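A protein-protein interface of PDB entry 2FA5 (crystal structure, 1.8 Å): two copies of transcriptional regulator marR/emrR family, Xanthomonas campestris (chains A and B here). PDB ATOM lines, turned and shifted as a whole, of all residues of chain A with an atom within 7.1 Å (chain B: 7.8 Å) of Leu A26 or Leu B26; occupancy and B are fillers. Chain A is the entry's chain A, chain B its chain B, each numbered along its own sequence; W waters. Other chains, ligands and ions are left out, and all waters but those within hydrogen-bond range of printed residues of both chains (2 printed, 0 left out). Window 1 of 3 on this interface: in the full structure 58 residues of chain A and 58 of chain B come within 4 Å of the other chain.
The side-chain hydroxyl of Ser A30 lies close to the backbone NH of Ser B27 (3.4 Å).
O of Pro B23 is in hydrogen-bond range of OG of Ser B27 (3.4 Å). The backbone carbonyl oxygen of Tyr B24 is in hydrogen-bond range of the side-chain hydroxyl of Ser B27, at 2.9 Å. The backbone carbonyl oxygen of Ser B27 sits close to the side-chain amide nitrogen of Asn B31, at 3.3 Å. O of Ser A27 sits close to OD1 of Asn A31, 3.4 Å away.
Among the printed residues, merely in contact across the chains: Pro A23 with Ile B33 (3.9 Å), Leu A26 with Leu B26 (3.6 Å), Leu A26 with Leu B29 (3.7 Å), Leu A26 with Ile B33 (3.9 Å), Ser A27 with Ser B30 (3.3 Å), Leu A29 with Ile B147 (3.8 Å), Ser A30 with Leu B26 (3.7 Å), Ile A33 with Pro B23 (3.8 Å), Ile A33 with Leu B26 (3.8 Å), Leu A131 with Leu B150 (3.7 Å), Leu A143 with Leu B150 (3.8 Å), Ile A147 with Leu B26 (3.8 Å), Ile A147 with Leu B29 (3.9 Å), Leu A150 with Leu B29 (3.8 Å) and Leu A150 with Leu B131 (3.4 Å).
Of chain B, only Leu B26, Leu B29 and Ile B33 come within 4 Å of Leu A26. Printed residues of chain B within 4 Å of Ser A30: Leu B26 (3.7 Å) and Ser B27 (3.2 Å). Arg B25 touches none of the printed residues of chain A. Printed residues of chain A within 4 Å of Leu B26: Leu A26, Ser A30, Ile A33 and Ile A147. Val B28 touches none of the printed residues of chain A. Printed residues of chain A within 4 Å of Ile B33: Pro A23 (3.9 Å) and Leu A26 (3.9 Å). The nearest residue of chain B that does not touch Leu A26 is Ile B147 (4.2 Å).
Of the 17 printed residues of chain A, 10 touch a printed residue of chain B. Along chain B the printed residues that touch a printed residue of chain A span positions 23 to 150. Among the printed residues, no Asp or Glu carboxylate lies within 4 Å of a Lys or Arg side-chain nitrogen of the other chain.
Leu A26 touches its own counterpart, Leu B26. Leu A26 touches Leu B29, but with the chains exchanged Leu A29 does not touch Leu B26 (4.4 Å). Ser A27 touches Ser B30, and with the chains exchanged Ser A30 touches Ser B27. Ser A30 touches Leu B26, but with the chains exchanged Leu A26 does not touch Ser B30 (4.2 Å). Of the 16 pairs that touch across the chains among the printed residues, 11 have their exchanged pair printed and touching as well.
Water W1 bridges the backbone carbonyl oxygen of Pro B23 (2.7 Å) and the side-chain hydroxyl of Ser A30 (2.9 Å). Water W2 bridges the side-chain hydroxyl of Ser B30 (2.8 Å) and the backbone carbonyl oxygen of Pro A23 (2.9 Å).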
ATOM      1  N   PHE A  21       1.358  11.974   3.976  1.00  0.00           N
ATOM      2  CA  PHE A  21       2.322  10.904   4.228  1.00  0.00           C
ATOM      3  C   PHE A  21       1.858  10.087   5.442  1.00  0.00           C
ATOM      4  O   PHE A  21       1.896  10.570   6.574  1.00  0.00           O
ATOM      5  CB  PHE A  21       3.696  11.540   4.489  1.00  0.00           C
ATOM      6  CG  PHE A  21       4.849  10.577   4.424  1.00  0.00           C
ATOM      7  CD1 PHE A  21       5.104   9.850   3.266  1.00  0.00           C
ATOM      8  CD2 PHE A  21       5.704  10.428   5.508  1.00  0.00           C
ATOM      9  CE1 PHE A  21       6.198   8.989   3.190  1.00  0.00           C
ATOM     10  CE2 PHE A  21       6.799   9.570   5.445  1.00  0.00           C
ATOM     11  CZ  PHE A  21       7.048   8.849   4.280  1.00  0.00           C
ATOM     12  N   LEU A  22       1.425   8.852   5.200  1.00  0.00           N
ATOM     13  CA  LEU A  22       0.919   7.983   6.265  1.00  0.00           C
ATOM     14  C   LEU A  22       1.739   7.946   7.562  1.00  0.00           C
ATOM     15  O   LEU A  22       1.182   8.104   8.649  1.00  0.00           O
ATOM     16  CB  LEU A  22       0.739   6.557   5.732  1.00  0.00           C
ATOM     17  CG  LEU A  22      -0.014   5.530   6.589  1.00  0.00           C
ATOM     18  CD1 LEU A  22       0.831   5.084   7.777  1.00  0.00           C
ATOM     19  CD2 LEU A  22      -1.335   6.130   7.039  1.00  0.00           C
ATOM     20  N   PRO A  23       3.060   7.718   7.474  1.00  0.00           N
ATOM     21  CA  PRO A  23       3.861   7.678   8.704  1.00  0.00           C
ATOM     22  C   PRO A  23       3.708   8.944   9.549  1.00  0.00           C
ATOM     23  O   PRO A  23       3.676   8.888  10.786  1.00  0.00           O
ATOM     24  CB  PRO A  23       5.284   7.494   8.180  1.00  0.00           C
ATOM     25  CG  PRO A  23       5.067   6.656   6.941  1.00  0.00           C
ATOM     26  CD  PRO A  23       3.878   7.354   6.302  1.00  0.00           C
ATOM     27  N   TYR A  24       3.617  10.084   8.876  1.00  0.00           N
ATOM     28  CA  TYR A  24       3.466  11.362   9.556  1.00  0.00           C
ATOM     29  C   TYR A  24       2.069  11.459  10.158  1.00  0.00           C
ATOM     30  O   TYR A  24       1.912  11.804  11.325  1.00  0.00           O
ATOM     31  CB  TYR A  24       3.688  12.513   8.571  1.00  0.00           C
ATOM     32  CG  TYR A  24       3.615  13.888   9.200  1.00  0.00           C
ATOM     33  CD1 TYR A  24       4.589  14.316  10.099  1.00  0.00           C
ATOM     34  CD2 TYR A  24       2.572  14.763   8.893  1.00  0.00           C
ATOM     35  CE1 TYR A  24       4.531  15.581  10.673  1.00  0.00           C
ATOM     36  CE2 TYR A  24       2.504  16.027   9.462  1.00  0.00           C
ATOM     37  CZ  TYR A  24       3.485  16.429  10.352  1.00  0.00           C
ATOM     38  OH  TYR A  24       3.423  17.681  10.924  1.00  0.00           O
ATOM     39  N   ARG A  25       1.058  11.159   9.349  1.00  0.00           N
ATOM     40  CA  ARG A  25      -0.327  11.211   9.800  1.00  0.00           C
ATOM     41  C   ARG A  25      -0.532  10.339  11.037  1.00  0.00           C
ATOM     42  O   ARG A  25      -1.211  10.741  11.986  1.00  0.00           O
ATOM     43  CB  ARG A  25      -1.262  10.752   8.676  1.00  0.00           C
ATOM     44  CG  ARG A  25      -1.398  11.743   7.521  1.00  0.00           C
ATOM     45  CD  ARG A  25      -2.595  12.678   7.706  1.00  0.00           C
ATOM     46  NE  ARG A  25      -2.487  13.530   8.891  1.00  0.00           N
ATOM     47  CZ  ARG A  25      -1.554  14.464   9.060  1.00  0.00           C
ATOM     48  NH1 ARG A  25      -0.640  14.671   8.120  1.00  0.00           N
ATOM     49  NH2 ARG A  25      -1.536  15.196  10.168  1.00  0.00           N
ATOM     50  N   LEU A  26       0.059   9.148  11.028  1.00  0.00           N
ATOM     51  CA  LEU A  26      -0.070   8.236  12.161  1.00  0.00           C
ATOM     52  C   LEU A  26       0.655   8.784  13.385  1.00  0.00           C
ATOM     53  O   LEU A  26       0.123   8.753  14.496  1.00  0.00           O
ATOM     54  CB  LEU A  26       0.503   6.862  11.817  1.00  0.00           C
ATOM     55  CG  LEU A  26       0.263   5.789  12.882  1.00  0.00           C
ATOM     56  CD1 LEU A  26      -1.229   5.495  12.966  1.00  0.00           C
ATOM     57  CD2 LEU A  26       1.038   4.523  12.534  1.00  0.00           C
ATOM     58  N   SER A  27       1.870   9.279  13.172  1.00  0.00           N
ATOM     59  CA  SER A  27       2.685   9.837  14.248  1.00  0.00           C
ATOM     60  C   SER A  27       1.986  11.015  14.920  1.00  0.00           C
ATOM     61  O   SER A  27       1.915  11.086  16.147  1.00  0.00           O
ATOM     62  CB  SER A  27       4.040  10.291  13.698  1.00  0.00           C
ATOM     63  OG  SER A  27       4.856  10.826  14.726  1.00  0.00           O
ATOM     64  N   VAL A  28       1.476  11.942  14.116  1.00  0.00           N
ATOM     65  CA  VAL A  28       0.786  13.105  14.659  1.00  0.00           C
ATOM     66  C   VAL A  28      -0.464  12.700  15.451  1.00  0.00           C
ATOM     67  O   VAL A  28      -0.671  13.172  16.569  1.00  0.00           O
ATOM     68  CB  VAL A  28       0.391  14.100  13.533  1.00  0.00           C
ATOM     69  CG1 VAL A  28      -0.401  15.271  14.108  1.00  0.00           C
ATOM     70  CG2 VAL A  28       1.652  14.618  12.846  1.00  0.00           C
ATOM     71  N   LEU A  29      -1.290  11.824  14.883  1.00  0.00           N
ATOM     72  CA  LEU A  29      -2.500  11.392  15.576  1.00  0.00           C
ATOM     73  C   LEU A  29      -2.171  10.711  16.899  1.00  0.00           C
ATOM     74  O   LEU A  29      -2.825  10.960  17.917  1.00  0.00           O
ATOM     75  CB  LEU A  29      -3.320  10.433  14.708  1.00  0.00           C
ATOM     76  CG  LEU A  29      -4.523   9.819  15.440  1.00  0.00           C
ATOM     77  CD1 LEU A  29      -5.492  10.931  15.843  1.00  0.00           C
ATOM     78  CD2 LEU A  29      -5.222   8.792  14.554  1.00  0.00           C
ATOM     79  N   SER A  30      -1.163   9.847  16.880  1.00  0.00           N
ATOM     80  CA  SER A  30      -0.744   9.133  18.085  1.00  0.00           C
ATOM     81  C   SER A  30      -0.267  10.124  19.152  1.00  0.00           C
ATOM     82  O   SER A  30      -0.602   9.995  20.331  1.00  0.00           O
ATOM     83  CB  SER A  30       0.386   8.158  17.747  1.00  0.00           C
ATOM     84  OG  SER A  30       0.878   7.541  18.921  1.00  0.00           O
ATOM     85  N   ASN A  31       0.514  11.115  18.727  1.00  0.00           N
ATOM     86  CA  ASN A  31       1.019  12.132  19.643  1.00  0.00           C
ATOM     87  C   ASN A  31      -0.120  12.959  20.247  1.00  0.00           C
ATOM     88  O   ASN A  31      -0.082  13.301  21.429  1.00  0.00           O
ATOM     89  CB  ASN A  31       2.004  13.065  18.924  1.00  0.00           C
ATOM     90  CG  ASN A  31       3.332  12.393  18.613  1.00  0.00           C
ATOM     91  OD1 ASN A  31       3.610  11.290  19.080  1.00  0.00           O
ATOM     92  ND2 ASN A  31       4.166  13.067  17.822  1.00  0.00           N
ATOM     93  N   ARG A  32      -1.132  13.276  19.444  1.00  0.00           N
ATOM     94  CA  ARG A  32      -2.264  14.061  19.937  1.00  0.00           C
ATOM     95  C   ARG A  32      -3.119  13.246  20.901  1.00  0.00           C
ATOM     96  O   ARG A  32      -3.583  13.767  21.915  1.00  0.00           O
ATOM     97  CB  ARG A  32      -3.114  14.585  18.774  1.00  0.00           C
ATOM     98  CG  ARG A  32      -2.414  15.661  17.945  1.00  0.00           C
ATOM     99  CD  ARG A  32      -3.305  16.182  16.822  1.00  0.00           C
ATOM    100  NE  ARG A  32      -4.374  17.047  17.319  1.00  0.00           N
ATOM    101  CZ  ARG A  32      -5.337  17.562  16.557  1.00  0.00           C
ATOM    102  NH1 ARG A  32      -5.377  17.297  15.258  1.00  0.00           N
ATOM    103  NH2 ARG A  32      -6.263  18.344  17.095  1.00  0.00           N
ATOM    104  N   ILE A  33      -3.340  11.973  20.582  1.00  0.00           N
ATOM    105  CA  ILE A  33      -4.103  11.100  21.473  1.00  0.00           C
ATOM    106  C   ILE A  33      -3.350  11.016  22.816  1.00  0.00           C
ATOM    107  O   ILE A  33      -3.934  11.199  23.887  1.00  0.00           O
ATOM    108  CB  ILE A  33      -4.251   9.680  20.869  1.00  0.00           C
ATOM    109  CG1 ILE A  33      -5.238   9.717  19.694  1.00  0.00           C
ATOM    110  CG2 ILE A  33      -4.731   8.692  21.931  1.00  0.00           C
ATOM    111  CD1 ILE A  33      -5.317   8.402  18.919  1.00  0.00           C
ATOM    112  N   LEU A 131     -13.019   8.706  22.921  1.00  0.00           N
ATOM    113  CA  LEU A 131     -12.320   8.851  21.650  1.00  0.00           C
ATOM    114  C   LEU A 131     -12.874   7.879  20.609  1.00  0.00           C
ATOM    115  O   LEU A 131     -13.148   8.261  19.474  1.00  0.00           O
ATOM    116  CB  LEU A 131     -10.819   8.583  21.835  1.00  0.00           C
ATOM    117  CG  LEU A 131     -10.004   8.284  20.570  1.00  0.00           C
ATOM    118  CD1 LEU A 131      -9.967   9.510  19.665  1.00  0.00           C
ATOM    119  CD2 LEU A 131      -8.591   7.864  20.961  1.00  0.00           C
ATOM    120  N   LEU A 143     -10.508  -0.858  11.971  1.00  0.00           N
ATOM    121  CA  LEU A 143      -9.302  -0.100  12.278  1.00  0.00           C
ATOM    122  C   LEU A 143      -8.249  -1.012  12.900  1.00  0.00           C
ATOM    123  O   LEU A 143      -7.082  -0.983  12.515  1.00  0.00           O
ATOM    124  CB  LEU A 143      -9.624   1.044  13.241  1.00  0.00           C
ATOM    125  CG  LEU A 143      -8.426   1.877  13.713  1.00  0.00           C
ATOM    126  CD1 LEU A 143      -7.714   2.488  12.516  1.00  0.00           C
ATOM    127  CD2 LEU A 143      -8.903   2.961  14.667  1.00  0.00           C
ATOM    128  N   ILE A 147      -4.512  -1.935  11.363  1.00  0.00           N
ATOM    129  CA  ILE A 147      -3.324  -1.650  12.166  1.00  0.00           C
ATOM    130  C   ILE A 147      -2.527  -2.940  12.327  1.00  0.00           C
ATOM    131  O   ILE A 147      -1.300  -2.942  12.215  1.00  0.00           O
ATOM    132  CB  ILE A 147      -3.695  -1.112  13.572  1.00  0.00           C
ATOM    133  CG1 ILE A 147      -4.411   0.235  13.445  1.00  0.00           C
ATOM    134  CG2 ILE A 147      -2.444  -0.966  14.426  1.00  0.00           C
ATOM    135  CD1 ILE A 147      -3.618   1.294  12.699  1.00  0.00           C
ATOM    136  N   LEU A 150      -0.656  -3.734   9.160  1.00  0.00           N
ATOM    137  CA  LEU A 150       0.474  -2.837   8.985  1.00  0.00           C
ATOM    138  C   LEU A 150       1.651  -3.316   9.835  1.00  0.00           C
ATOM    139  O   LEU A 150       2.798  -3.297   9.391  1.00  0.00           O
ATOM    140  CB  LEU A 150       0.064  -1.417   9.385  1.00  0.00           C
ATOM    141  CG  LEU A 150       0.883  -0.256   8.824  1.00  0.00           C
ATOM    142  CD1 LEU A 150       1.009  -0.397   7.313  1.00  0.00           C
ATOM    143  CD2 LEU A 150       0.206   1.057   9.190  1.00  0.00           C
ATOM    144  N   LEU B  18      -2.877  -3.164  27.659  1.00  0.00           N
ATOM    145  CA  LEU B  18      -2.115  -2.470  26.633  1.00  0.00           C
ATOM    146  C   LEU B  18      -2.121  -3.002  25.212  1.00  0.00           C
ATOM    147  O   LEU B  18      -2.345  -2.234  24.282  1.00  0.00           O
ATOM    148  CB  LEU B  18      -0.665  -2.309  27.092  1.00  0.00           C
ATOM    149  CG  LEU B  18      -0.476  -1.470  28.354  1.00  0.00           C
ATOM    150  CD1 LEU B  18       1.000  -1.435  28.712  1.00  0.00           C
ATOM    151  CD2 LEU B  18      -1.004  -0.056  28.128  1.00  0.00           C
ATOM    152  N   PHE B  21      -5.132  -1.937  23.541  1.00  0.00           N
ATOM    153  CA  PHE B  21      -5.477  -0.551  23.840  1.00  0.00           C
ATOM    154  C   PHE B  21      -4.997   0.328  22.682  1.00  0.00           C
ATOM    155  O   PHE B  21      -3.802   0.512  22.494  1.00  0.00           O
ATOM    156  CB  PHE B  21      -4.799  -0.132  25.150  1.00  0.00           C
ATOM    157  CG  PHE B  21      -5.295   1.171  25.705  1.00  0.00           C
ATOM    158  CD1 PHE B  21      -6.650   1.358  25.969  1.00  0.00           C
ATOM    159  CD2 PHE B  21      -4.407   2.204  25.985  1.00  0.00           C
ATOM    160  CE1 PHE B  21      -7.111   2.558  26.505  1.00  0.00           C
ATOM    161  CE2 PHE B  21      -4.859   3.412  26.523  1.00  0.00           C
ATOM    162  CZ  PHE B  21      -6.208   3.589  26.784  1.00  0.00           C
ATOM    163  N   LEU B  22      -5.942   0.870  21.917  1.00  0.00           N
ATOM    164  CA  LEU B  22      -5.639   1.696  20.747  1.00  0.00           C
ATOM    165  C   LEU B  22      -4.498   2.709  20.879  1.00  0.00           C
ATOM    166  O   LEU B  22      -3.591   2.736  20.045  1.00  0.00           O
ATOM    167  CB  LEU B  22      -6.905   2.425  20.282  1.00  0.00           C
ATOM    168  CG  LEU B  22      -7.260   2.326  18.797  1.00  0.00           C
ATOM    169  CD1 LEU B  22      -6.094   2.805  17.953  1.00  0.00           C
ATOM    170  CD2 LEU B  22      -7.608   0.884  18.452  1.00  0.00           C
ATOM    171  N   PRO B  23      -4.527   3.566  21.916  1.00  0.00           N
ATOM    172  CA  PRO B  23      -3.446   4.551  22.066  1.00  0.00           C
ATOM    173  C   PRO B  23      -2.060   3.907  22.132  1.00  0.00           C
ATOM    174  O   PRO B  23      -1.091   4.413  21.555  1.00  0.00           O
ATOM    175  CB  PRO B  23      -3.811   5.265  23.363  1.00  0.00           C
ATOM    176  CG  PRO B  23      -5.312   5.219  23.349  1.00  0.00           C
ATOM    177  CD  PRO B  23      -5.581   3.791  22.922  1.00  0.00           C
ATOM    178  N   TYR B  24      -1.974   2.793  22.843  1.00  0.00           N
ATOM    179  CA  TYR B  24      -0.717   2.071  22.989  1.00  0.00           C
ATOM    180  C   TYR B  24      -0.314   1.445  21.655  1.00  0.00           C
ATOM    181  O   TYR B  24       0.832   1.576  21.211  1.00  0.00           O
ATOM    182  CB  TYR B  24      -0.870   0.993  24.061  1.00  0.00           C
ATOM    183  CG  TYR B  24       0.356   0.137  24.261  1.00  0.00           C
ATOM    184  CD1 TYR B  24       0.497  -1.084  23.600  1.00  0.00           C
ATOM    185  CD2 TYR B  24       1.371   0.541  25.125  1.00  0.00           C
ATOM    186  CE1 TYR B  24       1.625  -1.887  23.803  1.00  0.00           C
ATOM    187  CE2 TYR B  24       2.497  -0.250  25.334  1.00  0.00           C
ATOM    188  CZ  TYR B  24       2.618  -1.462  24.674  1.00  0.00           C
ATOM    189  OH  TYR B  24       3.717  -2.253  24.921  1.00  0.00           O
ATOM    190  N   ARG B  25      -1.263   0.769  21.018  1.00  0.00           N
ATOM    191  CA  ARG B  25      -1.023   0.120  19.731  1.00  0.00           C
ATOM    192  C   ARG B  25      -0.523   1.116  18.686  1.00  0.00           C
ATOM    193  O   ARG B  25       0.395   0.817  17.922  1.00  0.00           O
ATOM    194  CB  ARG B  25      -2.311  -0.541  19.235  1.00  0.00           C
ATOM    195  CG  ARG B  25      -2.758  -1.727  20.068  1.00  0.00           C
ATOM    196  CD  ARG B  25      -2.225  -3.030  19.497  1.00  0.00           C
ATOM    197  NE  ARG B  25      -2.775  -3.300  18.169  1.00  0.00           N
ATOM    198  CZ  ARG B  25      -4.072  -3.430  17.908  1.00  0.00           C
ATOM    199  NH1 ARG B  25      -4.479  -3.675  16.669  1.00  0.00           N
ATOM    200  NH2 ARG B  25      -4.966  -3.317  18.880  1.00  0.00           N
ATOM    201  N   LEU B  26      -1.128   2.300  18.656  1.00  0.00           N
ATOM    202  CA  LEU B  26      -0.730   3.326  17.699  1.00  0.00           C
ATOM    203  C   LEU B  26       0.641   3.918  18.008  1.00  0.00           C
ATOM    204  O   LEU B  26       1.428   4.170  17.093  1.00  0.00           O
ATOM    205  CB  LEU B  26      -1.768   4.451  17.650  1.00  0.00           C
ATOM    206  CG  LEU B  26      -3.102   4.113  16.986  1.00  0.00           C
ATOM    207  CD1 LEU B  26      -3.999   5.340  17.023  1.00  0.00           C
ATOM    208  CD2 LEU B  26      -2.873   3.667  15.543  1.00  0.00           C
ATOM    209  N   SER B  27       0.928   4.155  19.287  1.00  0.00           N
ATOM    210  CA  SER B  27       2.223   4.721  19.657  1.00  0.00           C
ATOM    211  C   SER B  27       3.334   3.723  19.363  1.00  0.00           C
ATOM    212  O   SER B  27       4.386   4.095  18.852  1.00  0.00           O
ATOM    213  CB  SER B  27       2.253   5.108  21.145  1.00  0.00           C
ATOM    214  OG  SER B  27       2.216   3.964  21.978  1.00  0.00           O
ATOM    215  N   VAL B  28       3.111   2.450  19.682  1.00  0.00           N
ATOM    216  CA  VAL B  28       4.140   1.444  19.416  1.00  0.00           C
ATOM    217  C   VAL B  28       4.402   1.290  17.917  1.00  0.00           C
ATOM    218  O   VAL B  28       5.556   1.272  17.480  1.00  0.00           O
ATOM    219  CB  VAL B  28       3.756   0.070  20.017  1.00  0.00           C
ATOM    220  CG1 VAL B  28       4.774  -0.989  19.601  1.00  0.00           C
ATOM    221  CG2 VAL B  28       3.710   0.171  21.529  1.00  0.00           C
ATOM    222  N   LEU B  29       3.336   1.181  17.128  1.00  0.00           N
ATOM    223  CA  LEU B  29       3.489   1.036  15.680  1.00  0.00           C
ATOM    224  C   LEU B  29       4.229   2.237  15.097  1.00  0.00           C
ATOM    225  O   LEU B  29       5.124   2.080  14.272  1.00  0.00           O
ATOM    226  CB  LEU B  29       2.117   0.904  15.001  1.00  0.00           C
ATOM    227  CG  LEU B  29       2.127   0.889  13.464  1.00  0.00           C
ATOM    228  CD1 LEU B  29       2.928  -0.303  12.949  1.00  0.00           C
ATOM    229  CD2 LEU B  29       0.696   0.825  12.946  1.00  0.00           C
ATOM    230  N   SER B  30       3.852   3.439  15.526  1.00  0.00           N
ATOM    231  CA  SER B  30       4.500   4.647  15.028  1.00  0.00           C
ATOM    232  C   SER B  30       5.991   4.644  15.371  1.00  0.00           C
ATOM    233  O   SER B  30       6.817   5.033  14.548  1.00  0.00           O
ATOM    234  CB  SER B  30       3.825   5.890  15.618  1.00  0.00           C
ATOM    235  OG  SER B  30       4.364   7.066  15.053  1.00  0.00           O
ATOM    236  N   ASN B  31       6.327   4.213  16.589  1.00  0.00           N
ATOM    237  CA  ASN B  31       7.723   4.134  17.035  1.00  0.00           C
ATOM    238  C   ASN B  31       8.518   3.194  16.120  1.00  0.00           C
ATOM    239  O   ASN B  31       9.650   3.488  15.730  1.00  0.00           O
ATOM    240  CB  ASN B  31       7.807   3.580  18.463  1.00  0.00           C
ATOM    241  CG  ASN B  31       7.367   4.580  19.525  1.00  0.00           C
ATOM    242  OD1 ASN B  31       7.232   4.225  20.698  1.00  0.00           O
ATOM    243  ND2 ASN B  31       7.157   5.823  19.128  1.00  0.00           N
ATOM    244  N   ARG B  32       7.923   2.051  15.794  1.00  0.00           N
ATOM    245  CA  ARG B  32       8.590   1.076  14.933  1.00  0.00           C
ATOM    246  C   ARG B  32       8.762   1.604  13.514  1.00  0.00           C
ATOM    247  O   ARG B  32       9.814   1.411  12.907  1.00  0.00           O
ATOM    248  CB  ARG B  32       7.815  -0.248  14.920  1.00  0.00           C
ATOM    249  CG  ARG B  32       7.806  -0.966  16.265  1.00  0.00           C
ATOM    250  CD  ARG B  32       7.146  -2.340  16.190  1.00  0.00           C
ATOM    251  NE  ARG B  32       6.912  -2.914  17.516  1.00  0.00           N
ATOM    252  CZ  ARG B  32       7.873  -3.244  18.378  1.00  0.00           C
ATOM    253  NH1 ARG B  32       9.148  -3.062  18.057  1.00  0.00           N
ATOM    254  NH2 ARG B  32       7.558  -3.748  19.565  1.00  0.00           N
ATOM    255  N   ILE B  33       7.735   2.270  12.984  1.00  0.00           N
ATOM    256  CA  ILE B  33       7.817   2.831  11.634  1.00  0.00           C
ATOM    257  C   ILE B  33       8.930   3.887  11.581  1.00  0.00           C
ATOM    258  O   ILE B  33       9.757   3.887  10.669  1.00  0.00           O
ATOM    259  CB  ILE B  33       6.466   3.471  11.209  1.00  0.00           C
ATOM    260  CG1 ILE B  33       5.424   2.367  10.990  1.00  0.00           C
ATOM    261  CG2 ILE B  33       6.644   4.302   9.933  1.00  0.00           C
ATOM    262  CD1 ILE B  33       4.027   2.890  10.665  1.00  0.00           C
ATOM    263  N   LEU B 131       5.992  -0.147   2.743  1.00  0.00           N
ATOM    264  CA  LEU B 131       5.124  -0.311   3.908  1.00  0.00           C
ATOM    265  C   LEU B 131       3.648  -0.407   3.525  1.00  0.00           C
ATOM    266  O   LEU B 131       2.930  -1.288   4.004  1.00  0.00           O
ATOM    267  CB  LEU B 131       5.301   0.866   4.877  1.00  0.00           C
ATOM    268  CG  LEU B 131       4.270   0.993   6.011  1.00  0.00           C
ATOM    269  CD1 LEU B 131       4.425  -0.169   6.997  1.00  0.00           C
ATOM    270  CD2 LEU B 131       4.458   2.332   6.733  1.00  0.00           C
ATOM    271  N   LEU B 143      -8.098   3.200   5.776  1.00  0.00           N
ATOM    272  CA  LEU B 143      -7.264   3.542   6.925  1.00  0.00           C
ATOM    273  C   LEU B 143      -7.171   5.056   7.087  1.00  0.00           C
ATOM    274  O   LEU B 143      -7.443   5.595   8.160  1.00  0.00           O
ATOM    275  CB  LEU B 143      -5.856   2.958   6.760  1.00  0.00           C
ATOM    276  CG  LEU B 143      -4.872   3.310   7.882  1.00  0.00           C
ATOM    277  CD1 LEU B 143      -5.451   2.872   9.220  1.00  0.00           C
ATOM    278  CD2 LEU B 143      -3.531   2.634   7.636  1.00  0.00           C
ATOM    279  N   ILE B 147      -8.461   7.268  10.187  1.00  0.00           N
ATOM    280  CA  ILE B 147      -7.513   8.113  10.905  1.00  0.00           C
ATOM    281  C   ILE B 147      -8.010   9.557  10.928  1.00  0.00           C
ATOM    282  O   ILE B 147      -7.944  10.229  11.960  1.00  0.00           O
ATOM    283  CB  ILE B 147      -6.105   8.084  10.252  1.00  0.00           C
ATOM    284  CG1 ILE B 147      -5.423   6.744  10.537  1.00  0.00           C
ATOM    285  CG2 ILE B 147      -5.259   9.241  10.772  1.00  0.00           C
ATOM    286  CD1 ILE B 147      -4.001   6.657  10.010  1.00  0.00           C
ATOM    287  N   LEU B 150     -10.774   9.976  13.466  1.00  0.00           N
ATOM    288  CA  LEU B 150     -10.287  10.018  14.842  1.00  0.00           C
ATOM    289  C   LEU B 150      -9.708  11.388  15.158  1.00  0.00           C
ATOM    290  O   LEU B 150      -9.926  11.932  16.243  1.00  0.00           O
ATOM    291  CB  LEU B 150      -9.205   8.959  15.072  1.00  0.00           C
ATOM    292  CG  LEU B 150      -9.688   7.542  15.371  1.00  0.00           C
ATOM    293  CD1 LEU B 150      -8.486   6.625  15.581  1.00  0.00           C
ATOM    294  CD2 LEU B 150     -10.566   7.563  16.618  1.00  0.00           C
HETATM  295  O   HOH W   1      -1.199   7.003  20.810  1.00  0.00           O
HETATM  296  O   HOH W   2       4.962   6.794  12.297  1.00  0.00           O
